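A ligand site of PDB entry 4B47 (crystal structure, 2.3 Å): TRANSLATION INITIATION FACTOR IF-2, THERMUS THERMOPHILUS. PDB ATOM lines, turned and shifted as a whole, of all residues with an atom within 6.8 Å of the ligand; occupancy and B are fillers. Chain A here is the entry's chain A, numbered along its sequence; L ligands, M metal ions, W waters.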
ATOM      1  N   MET A  79      11.718  27.292   4.451  1.00  0.00           N
ATOM      2  CA  MET A  79      12.222  25.930   4.695  1.00  0.00           C
ATOM      3  C   MET A  79      11.126  24.875   4.677  1.00  0.00           C
ATOM      4  O   MET A  79       9.964  25.177   4.370  1.00  0.00           O
ATOM      5  CB  MET A  79      12.988  25.884   6.017  1.00  0.00           C
ATOM      6  CG  MET A  79      14.271  26.714   6.023  1.00  0.00           C
ATOM      7  SD  MET A  79      15.125  26.747   7.613  1.00  0.00           S
ATOM      8  CE  MET A  79      15.862  25.109   7.627  1.00  0.00           C
ATOM      9  N   GLY A  80      11.485  23.647   5.035  1.00  0.00           N
ATOM     10  CA  GLY A  80      10.575  22.513   4.986  1.00  0.00           C
ATOM     11  C   GLY A  80      10.816  21.441   3.927  1.00  0.00           C
ATOM     12  O   GLY A  80      11.615  21.616   3.003  1.00  0.00           O
ATOM     13  N   HIS A  81      10.109  20.330   4.078  1.00  0.00           N
ATOM     14  CA  HIS A  81      10.258  19.122   3.263  1.00  0.00           C
ATOM     15  C   HIS A  81      10.110  19.371   1.764  1.00  0.00           C
ATOM     16  O   HIS A  81       9.341  20.231   1.332  1.00  0.00           O
ATOM     17  CB  HIS A  81       9.225  18.092   3.731  1.00  0.00           C
ATOM     18  CG  HIS A  81       9.363  16.740   3.088  1.00  0.00           C
ATOM     19  ND1 HIS A  81       8.965  16.485   1.790  1.00  0.00           N
ATOM     20  CD2 HIS A  81       9.789  15.555   3.584  1.00  0.00           C
ATOM     21  CE1 HIS A  81       9.172  15.208   1.507  1.00  0.00           C
ATOM     22  NE2 HIS A  81       9.674  14.626   2.582  1.00  0.00           N
ATOM     23  N   VAL A  82      10.858  18.615   0.959  1.00  0.00           N
ATOM     24  CA  VAL A  82      10.816  18.732  -0.491  1.00  0.00           C
ATOM     25  C   VAL A  82       9.395  18.480  -1.013  1.00  0.00           C
ATOM     26  O   VAL A  82       8.633  17.719  -0.419  1.00  0.00           O
ATOM     27  CB  VAL A  82      11.837  17.771  -1.165  1.00  0.00           C
ATOM     28  CG1 VAL A  82      11.416  16.305  -0.983  1.00  0.00           C
ATOM     29  CG2 VAL A  82      12.001  18.106  -2.635  1.00  0.00           C
ATOM     30  N   ASP A  83       9.036  19.178  -2.092  1.00  0.00           N
ATOM     31  CA  ASP A  83       7.710  19.099  -2.726  1.00  0.00           C
ATOM     32  C   ASP A  83       6.602  19.825  -1.955  1.00  0.00           C
ATOM     33  O   ASP A  83       5.460  19.878  -2.406  1.00  0.00           O
ATOM     34  CB  ASP A  83       7.288  17.658  -3.017  1.00  0.00           C
ATOM     35  CG  ASP A  83       8.276  16.937  -3.929  1.00  0.00           C
ATOM     36  OD1 ASP A  83       8.908  17.608  -4.764  1.00  0.00           O
ATOM     37  OD2 ASP A  83       8.416  15.700  -3.794  1.00  0.00           O
ATOM     38  N   HIS A  84       6.945  20.373  -0.793  1.00  0.00           N
ATOM     39  CA  HIS A  84       5.950  21.086   0.018  1.00  0.00           C
ATOM     40  C   HIS A  84       5.615  22.487  -0.483  1.00  0.00           C
ATOM     41  O   HIS A  84       4.704  23.131   0.033  1.00  0.00           O
ATOM     42  CB  HIS A  84       6.330  21.090   1.499  1.00  0.00           C
ATOM     43  CG  HIS A  84       6.069  19.775   2.169  1.00  0.00           C
ATOM     44  ND1 HIS A  84       5.732  19.676   3.503  1.00  0.00           N
ATOM     45  CD2 HIS A  84       6.081  18.510   1.691  1.00  0.00           C
ATOM     46  CE1 HIS A  84       5.551  18.399   3.814  1.00  0.00           C
ATOM     47  NE2 HIS A  84       5.761  17.674   2.736  1.00  0.00           N
ATOM     48  N   GLY A  85       6.330  22.949  -1.513  1.00  0.00           N
ATOM     49  CA  GLY A  85       6.038  24.242  -2.114  1.00  0.00           C
ATOM     50  C   GLY A  85       6.968  25.423  -1.873  1.00  0.00           C
ATOM     51  O   GLY A  85       6.602  26.555  -2.227  1.00  0.00           O
ATOM     52  N   LYS A  86       8.139  25.186  -1.279  1.00  0.00           N
ATOM     53  CA  LYS A  86       9.094  26.268  -1.011  1.00  0.00           C
ATOM     54  C   LYS A  86       9.348  27.114  -2.253  1.00  0.00           C
ATOM     55  O   LYS A  86       9.209  28.334  -2.229  1.00  0.00           O
ATOM     56  CB  LYS A  86      10.417  25.699  -0.506  1.00  0.00           C
ATOM     57  CG  LYS A  86      10.305  24.856   0.767  1.00  0.00           C
ATOM     58  CD  LYS A  86      11.612  24.135   1.082  1.00  0.00           C
ATOM     59  CE  LYS A  86      11.954  23.084   0.029  1.00  0.00           C
ATOM     60  NZ  LYS A  86      13.105  22.226   0.400  1.00  0.00           N
ATOM     61  N   THR A  87       9.726  26.456  -3.351  1.00  0.00           N
ATOM     62  CA  THR A  87      10.033  27.145  -4.602  1.00  0.00           C
ATOM     63  C   THR A  87       8.826  27.892  -5.166  1.00  0.00           C
ATOM     64  O   THR A  87       8.951  29.012  -5.657  1.00  0.00           O
ATOM     65  CB  THR A  87      10.557  26.180  -5.697  1.00  0.00           C
ATOM     66  OG1 THR A  87      11.676  25.444  -5.201  1.00  0.00           O
ATOM     67  CG2 THR A  87      10.964  26.960  -6.931  1.00  0.00           C
ATOM     68  N   THR A  88       7.651  27.260  -5.093  1.00  0.00           N
ATOM     69  CA  THR A  88       6.433  27.868  -5.606  1.00  0.00           C
ATOM     70  C   THR A  88       6.094  29.141  -4.837  1.00  0.00           C
ATOM     71  O   THR A  88       5.658  30.132  -5.425  1.00  0.00           O
ATOM     72  CB  THR A  88       5.241  26.894  -5.521  1.00  0.00           C
ATOM     73  OG1 THR A  88       5.615  25.629  -6.069  1.00  0.00           O
ATOM     74  CG2 THR A  88       4.045  27.431  -6.279  1.00  0.00           C
ATOM     75  N   LEU A  89       6.311  29.104  -3.529  1.00  0.00           N
ATOM     76  CA  LEU A  89       6.019  30.257  -2.688  1.00  0.00           C
ATOM     77  C   LEU A  89       6.950  31.418  -2.998  1.00  0.00           C
ATOM     78  O   LEU A  89       6.505  32.555  -3.116  1.00  0.00           O
ATOM     79  CB  LEU A  89       6.109  29.876  -1.205  1.00  0.00           C
ATOM     80  CG  LEU A  89       5.902  31.010  -0.190  1.00  0.00           C
ATOM     81  CD1 LEU A  89       4.551  31.678  -0.388  1.00  0.00           C
ATOM     82  CD2 LEU A  89       6.060  30.495   1.232  1.00  0.00           C
ATOM     83  N   HIS A 130      20.836  23.886   0.284  1.00  0.00           N
ATOM     84  CA  HIS A 130      20.157  23.614   1.543  1.00  0.00           C
ATOM     85  C   HIS A 130      21.127  23.493   2.710  1.00  0.00           C
ATOM     86  O   HIS A 130      22.323  23.729   2.575  1.00  0.00           O
ATOM     87  CB  HIS A 130      19.310  22.350   1.439  1.00  0.00           C
ATOM     88  CG  HIS A 130      18.029  22.535   0.672  1.00  0.00           C
ATOM     89  ND1 HIS A 130      17.989  22.614  -0.703  1.00  0.00           N
ATOM     90  CD2 HIS A 130      16.749  22.673   1.094  1.00  0.00           C
ATOM     91  CE1 HIS A 130      16.743  22.777  -1.093  1.00  0.00           C
ATOM     92  NE2 HIS A 130      15.965  22.823  -0.020  1.00  0.00           N
ATOM     93  N   VAL A 150       7.298  25.670   5.723  1.00  0.00           N
ATOM     94  CA  VAL A 150       6.196  25.327   4.843  1.00  0.00           C
ATOM     95  C   VAL A 150       5.806  23.880   5.029  1.00  0.00           C
ATOM     96  O   VAL A 150       6.666  22.990   5.050  1.00  0.00           O
ATOM     97  CB  VAL A 150       6.580  25.544   3.367  1.00  0.00           C
ATOM     98  CG1 VAL A 150       5.376  25.279   2.473  1.00  0.00           C
ATOM     99  CG2 VAL A 150       7.098  26.953   3.150  1.00  0.00           C
ATOM    100  N   ASN A 180       0.520  24.833   3.541  1.00  0.00           N
ATOM    101  CA  ASN A 180       0.394  25.123   2.123  1.00  0.00           C
ATOM    102  C   ASN A 180      -0.577  24.140   1.486  1.00  0.00           C
ATOM    103  O   ASN A 180      -1.047  23.226   2.150  1.00  0.00           O
ATOM    104  CB  ASN A 180       1.779  25.028   1.470  1.00  0.00           C
ATOM    105  CG  ASN A 180       1.778  25.533   0.042  1.00  0.00           C
ATOM    106  OD1 ASN A 180       0.980  26.386  -0.330  1.00  0.00           O
ATOM    107  ND2 ASN A 180       2.682  24.997  -0.773  1.00  0.00           N
ATOM    108  N   LYS A 181      -0.852  24.339   0.194  1.00  0.00           N
ATOM    109  CA  LYS A 181      -1.731  23.465  -0.562  1.00  0.00           C
ATOM    110  C   LYS A 181      -3.096  23.282   0.104  1.00  0.00           C
ATOM    111  O   LYS A 181      -3.584  22.162   0.229  1.00  0.00           O
ATOM    112  CB  LYS A 181      -1.074  22.100  -0.785  1.00  0.00           C
ATOM    113  CG  LYS A 181       0.346  22.185  -1.304  1.00  0.00           C
ATOM    114  CD  LYS A 181       0.854  20.824  -1.758  1.00  0.00           C
ATOM    115  CE  LYS A 181       2.261  20.928  -2.316  1.00  0.00           C
ATOM    116  NZ  LYS A 181       2.669  19.702  -3.036  1.00  0.00           N
ATOM    117  N   ILE A 182      -3.693  24.395   0.547  1.00  0.00           N
ATOM    118  CA  ILE A 182      -5.019  24.342   1.159  1.00  0.00           C
ATOM    119  C   ILE A 182      -6.089  24.270   0.073  1.00  0.00           C
ATOM    120  O   ILE A 182      -7.254  23.977   0.349  1.00  0.00           O
ATOM    121  CB  ILE A 182      -5.293  25.542   2.088  1.00  0.00           C
ATOM    122  CG1 ILE A 182      -5.310  26.849   1.290  1.00  0.00           C
ATOM    123  CG2 ILE A 182      -4.293  25.610   3.233  1.00  0.00           C
ATOM    124  CD1 ILE A 182      -5.751  28.050   2.081  1.00  0.00           C
ATOM    125  N   ASP A 183      -5.676  24.533  -1.161  1.00  0.00           N
ATOM    126  CA  ASP A 183      -6.582  24.450  -2.306  1.00  0.00           C
ATOM    127  C   ASP A 183      -6.992  23.000  -2.567  1.00  0.00           C
ATOM    128  O   ASP A 183      -8.100  22.736  -3.050  1.00  0.00           O
ATOM    129  CB  ASP A 183      -5.903  25.040  -3.538  1.00  0.00           C
ATOM    130  CG  ASP A 183      -4.488  24.545  -3.706  1.00  0.00           C
ATOM    131  OD1 ASP A 183      -3.611  24.990  -2.941  1.00  0.00           O
ATOM    132  OD2 ASP A 183      -4.246  23.714  -4.602  1.00  0.00           O
ATOM    133  N   LEU A 184      -6.089  22.076  -2.256  1.00  0.00           N
ATOM    134  CA  LEU A 184      -6.329  20.658  -2.522  1.00  0.00           C
ATOM    135  C   LEU A 184      -7.536  20.133  -1.758  1.00  0.00           C
ATOM    136  O   LEU A 184      -7.789  20.550  -0.626  1.00  0.00           O
ATOM    137  CB  LEU A 184      -5.073  19.840  -2.187  1.00  0.00           C
ATOM    138  CG  LEU A 184      -3.817  20.143  -3.009  1.00  0.00           C
ATOM    139  CD1 LEU A 184      -2.717  19.130  -2.701  1.00  0.00           C
ATOM    140  CD2 LEU A 184      -4.128  20.151  -4.499  1.00  0.00           C
ATOM    141  N   ILE A 215      -2.031  28.726   3.652  1.00  0.00           N
ATOM    142  CA  ILE A 215      -1.724  29.379   2.373  1.00  0.00           C
ATOM    143  C   ILE A 215      -1.911  28.453   1.177  1.00  0.00           C
ATOM    144  O   ILE A 215      -1.845  27.234   1.292  1.00  0.00           O
ATOM    145  CB  ILE A 215      -0.277  29.928   2.313  1.00  0.00           C
ATOM    146  CG1 ILE A 215       0.736  28.798   2.489  1.00  0.00           C
ATOM    147  CG2 ILE A 215      -0.061  31.035   3.333  1.00  0.00           C
ATOM    148  CD1 ILE A 215       2.163  29.205   2.157  1.00  0.00           C
ATOM    149  N   SER A 216      -2.158  29.054   0.018  1.00  0.00           N
ATOM    150  CA  SER A 216      -2.042  28.338  -1.244  1.00  0.00           C
ATOM    151  C   SER A 216      -1.024  29.052  -2.128  1.00  0.00           C
ATOM    152  O   SER A 216      -1.283  30.144  -2.627  1.00  0.00           O
ATOM    153  CB  SER A 216      -3.393  28.250  -1.945  1.00  0.00           C
ATOM    154  OG  SER A 216      -3.263  27.614  -3.207  1.00  0.00           O
ATOM    155  N   ALA A 217       0.120  28.422  -2.344  1.00  0.00           N
ATOM    156  CA  ALA A 217       1.159  29.030  -3.169  1.00  0.00           C
ATOM    157  C   ALA A 217       0.735  29.025  -4.634  1.00  0.00           C
ATOM    158  O   ALA A 217       1.224  29.822  -5.436  1.00  0.00           O
ATOM    159  CB  ALA A 217       2.475  28.289  -2.992  1.00  0.00           C
ATOM    160  N   LYS A 218      -0.171  28.112  -4.968  1.00  0.00           N
ATOM    161  CA  LYS A 218      -0.737  28.037  -6.306  1.00  0.00           C
ATOM    162  C   LYS A 218      -1.671  29.220  -6.534  1.00  0.00           C
ATOM    163  O   LYS A 218      -1.525  29.979  -7.496  1.00  0.00           O
ATOM    164  CB  LYS A 218      -1.525  26.735  -6.471  1.00  0.00           C
ATOM    165  CG  LYS A 218      -1.869  26.353  -7.904  1.00  0.00           C
ATOM    166  CD  LYS A 218      -2.956  25.273  -7.939  1.00  0.00           C
ATOM    167  CE  LYS A 218      -2.980  24.508  -9.251  1.00  0.00           C
ATOM    168  NZ  LYS A 218      -2.187  23.253  -9.201  1.00  0.00           N
ATOM    169  N   THR A 219      -2.621  29.382  -5.611  1.00  0.00           N
ATOM    170  CA  THR A 219      -3.661  30.401  -5.725  1.00  0.00           C
ATOM    171  C   THR A 219      -3.196  31.789  -5.289  1.00  0.00           C
ATOM    172  O   THR A 219      -3.510  32.783  -5.946  1.00  0.00           O
ATOM    173  CB  THR A 219      -4.905  30.005  -4.890  1.00  0.00           C
ATOM    174  OG1 THR A 219      -5.440  28.777  -5.403  1.00  0.00           O
ATOM    175  CG2 THR A 219      -5.969  31.085  -4.955  1.00  0.00           C
ATOM    176  N   GLY A 220      -2.443  31.841  -4.203  1.00  0.00           N
ATOM    177  CA  GLY A 220      -2.058  33.112  -3.619  1.00  0.00           C
ATOM    178  C   GLY A 220      -2.909  33.442  -2.408  1.00  0.00           C
ATOM    179  O   GLY A 220      -2.779  34.514  -1.807  1.00  0.00           O
HETATM  180  P1  LIG L   1       9.656  22.557  -2.930  1.00  0.00           P
HETATM  181  O1  LIG L   1      10.636  21.411  -3.024  1.00  0.00           O
HETATM  182  O2  LIG L   1       9.269  22.764  -1.490  1.00  0.00           O
HETATM  183  O3  LIG L   1      10.280  23.795  -3.503  1.00  0.00           O
HETATM  184  O4  LIG L   1       8.322  22.203  -3.762  1.00  0.00           O
HETATM  185  P2  LIG L   1       7.961  22.992  -5.108  1.00  0.00           P
HETATM  186  O5  LIG L   1       7.805  24.463  -4.793  1.00  0.00           O
HETATM  187  O6  LIG L   1       8.985  22.768  -6.193  1.00  0.00           O
HETATM  188  O7  LIG L   1       6.539  22.356  -5.498  1.00  0.00           O
HETATM  189  C1  LIG L   1       6.461  21.053  -6.074  1.00  0.00           C
HETATM  190  C2  LIG L   1       5.049  20.849  -6.587  1.00  0.00           C
HETATM  191  O8  LIG L   1       4.114  21.251  -5.578  1.00  0.00           O
HETATM  192  C3  LIG L   1       4.791  21.719  -7.802  1.00  0.00           C
HETATM  193  O9  LIG L   1       4.305  20.906  -8.879  1.00  0.00           O
HETATM  194  C4  LIG L   1       3.715  22.708  -7.391  1.00  0.00           C
HETATM  195  O10 LIG L   1       2.742  22.870  -8.420  1.00  0.00           O
HETATM  196  C5  LIG L   1       3.087  22.056  -6.161  1.00  0.00           C
HETATM  197  N1  LIG L   1       2.586  23.096  -5.229  1.00  0.00           N
HETATM  198  C6  LIG L   1       3.323  23.929  -4.473  1.00  0.00           C
HETATM  199  N2  LIG L   1       2.522  24.746  -3.740  1.00  0.00           N
HETATM  200  C7  LIG L   1       1.243  24.432  -4.029  1.00  0.00           C
HETATM  201  C8  LIG L   1      -0.102  24.894  -3.614  1.00  0.00           C
HETATM  202  O11 LIG L   1      -0.237  25.817  -2.785  1.00  0.00           O
HETATM  203  N3  LIG L   1      -1.177  24.300  -4.164  1.00  0.00           N
HETATM  204  C9  LIG L   1      -1.057  23.309  -5.063  1.00  0.00           C
HETATM  205  N4  LIG L   1      -2.182  22.752  -5.575  1.00  0.00           N
HETATM  206  N5  LIG L   1       0.139  22.832  -5.490  1.00  0.00           N
HETATM  207  C10 LIG L   1       1.293  23.345  -5.010  1.00  0.00           C
HETATM  208 MG    MG M   1      11.719  22.522  -5.567  1.00  0.00          MG
HETATM  209  O   HOH W   1      13.461  23.867  -3.131  1.00  0.00           O
HETATM  210  O   HOH W   2       0.922  24.435  -8.872  1.00  0.00           O
HETATM  211  O   HOH W   3      10.386  19.864  -5.694  1.00  0.00           O
HETATM  212  O   HOH W   4      13.906  21.461  -3.420  1.00  0.00           O
HETATM  213  O   HOH W   5       3.408  18.772 -11.360  1.00  0.00           O
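A nitrogen (N4) of the ligand lies within hydrogen-bond range of the side-chain carboxylate (OD2) of Asp 183 (2.5 Å).
O11 of the ligand sits at hydrogen-bond distance from N of Ala 217 (2.7 Å).
The backbone NH (N) of Lys 86 is in hydrogen-bond range of an oxygen (O2) of the ligand.
N of Thr 87 sits at hydrogen-bond distance from O3 of the ligand (2.7 Å).
The side-chain hydroxyl (OG1) of Thr 87 sits at hydrogen-bond distance from an oxygen (O3) of the ligand (2.7 Å).
The backbone NH (N) of Thr 88 lies within hydrogen-bond range of an oxygen (O5) of the ligand (2.8 Å).
OG1 of Thr 88 sits at hydrogen-bond distance from O5 of the ligand (2.8 Å).
An oxygen (O11) of the ligand sits close to the side-chain amide oxygen (OD1) of Asn 180 (2.8 Å).
The backbone NH (N) of Asp 83 sits at hydrogen-bond distance from an oxygen (O1) of the ligand (2.9 Å).
The backbone NH (N) of Gly 85 sits at hydrogen-bond distance from an oxygen (O2) of the ligand, at 2.9 Å.
The backbone NH of Lys 218 sits at hydrogen-bond distance from an oxygen (O11) of the ligand, at 3.2 Å.
N of Lys 181 lies within hydrogen-bond range of O11 of the ligand (3.4 Å).
NZ of Lys 181 is in hydrogen-bond range of O8 of the ligand (3.3 Å).
An oxygen (O2) of the ligand lies within hydrogen-bond range of the backbone NH (N) of His 84 (3.4 Å).
The backbone NH (N) of Ala 217 is in hydrogen-bond range of the side-chain amide oxygen (OD1) of Asn 180, 3.0 Å away.
NZ of Lys 86 is in hydrogen-bond range of O of Gly 80, 3.1 Å away.
A ring nitrogen (NE2) of His 130 is in hydrogen-bond range of the side-chain amino group (NZ) of Lys 86 (3.0 Å).
The side-chain amide nitrogen of Asn 180 sits at hydrogen-bond distance from the backbone carbonyl oxygen of His 84, 2.9 Å away.
The backbone carbonyl oxygen (O) of Ile 215 sits close to the side-chain amide oxygen (OD1) of Asn 180, at 3.4 Å.
The backbone carbonyl oxygen of Asp 83 sits at hydrogen-bond distance from the side-chain amino group of Lys 181 (2.9 Å).
The backbone NH of Lys 181 lies within hydrogen-bond range of the backbone carbonyl oxygen of Ile 215, at 3.3 Å.
The backbone NH (N) of Thr 219 sits at hydrogen-bond distance from the side-chain hydroxyl (OG) of Ser 216, at 3.1 Å.
His 81 touches the ligand.
Val 82 touches the ligand.
Leu 184 touches the ligand (CD2 to N4, 3.4 Å).
Ser 216 touches the ligand (C to O11, 3.4 Å).
Hydrophobic or aromatic side chains that line the ligand: Val 82, Leu 184 and Ala 217.
15 residues have an atom within 4 Å of the ligand: His 81, Val 82, Asp 83, His 84, Gly 85, Lys 86, Thr 87, Thr 88, Asn 180, Lys 181, Asp 183, Leu 184, Ser 216, Ala 217 and Lys 218.
Along chain A the residues within 4 Å of the ligand span positions 81 to 218.
Water W2 bridges an oxygen (O10) of the ligand (2.4 Å) and the side-chain amino group (NZ) of Lys 218 (3.3 Å).
Water W3 bridges OD1 of Asp 83 (2.9 Å) and O1 of the ligand (3.1 Å).
Water W1 lies within hydrogen-bond range of the side-chain hydroxyl (OG1) of Thr 87 and an oxygen (O3) of the ligand.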
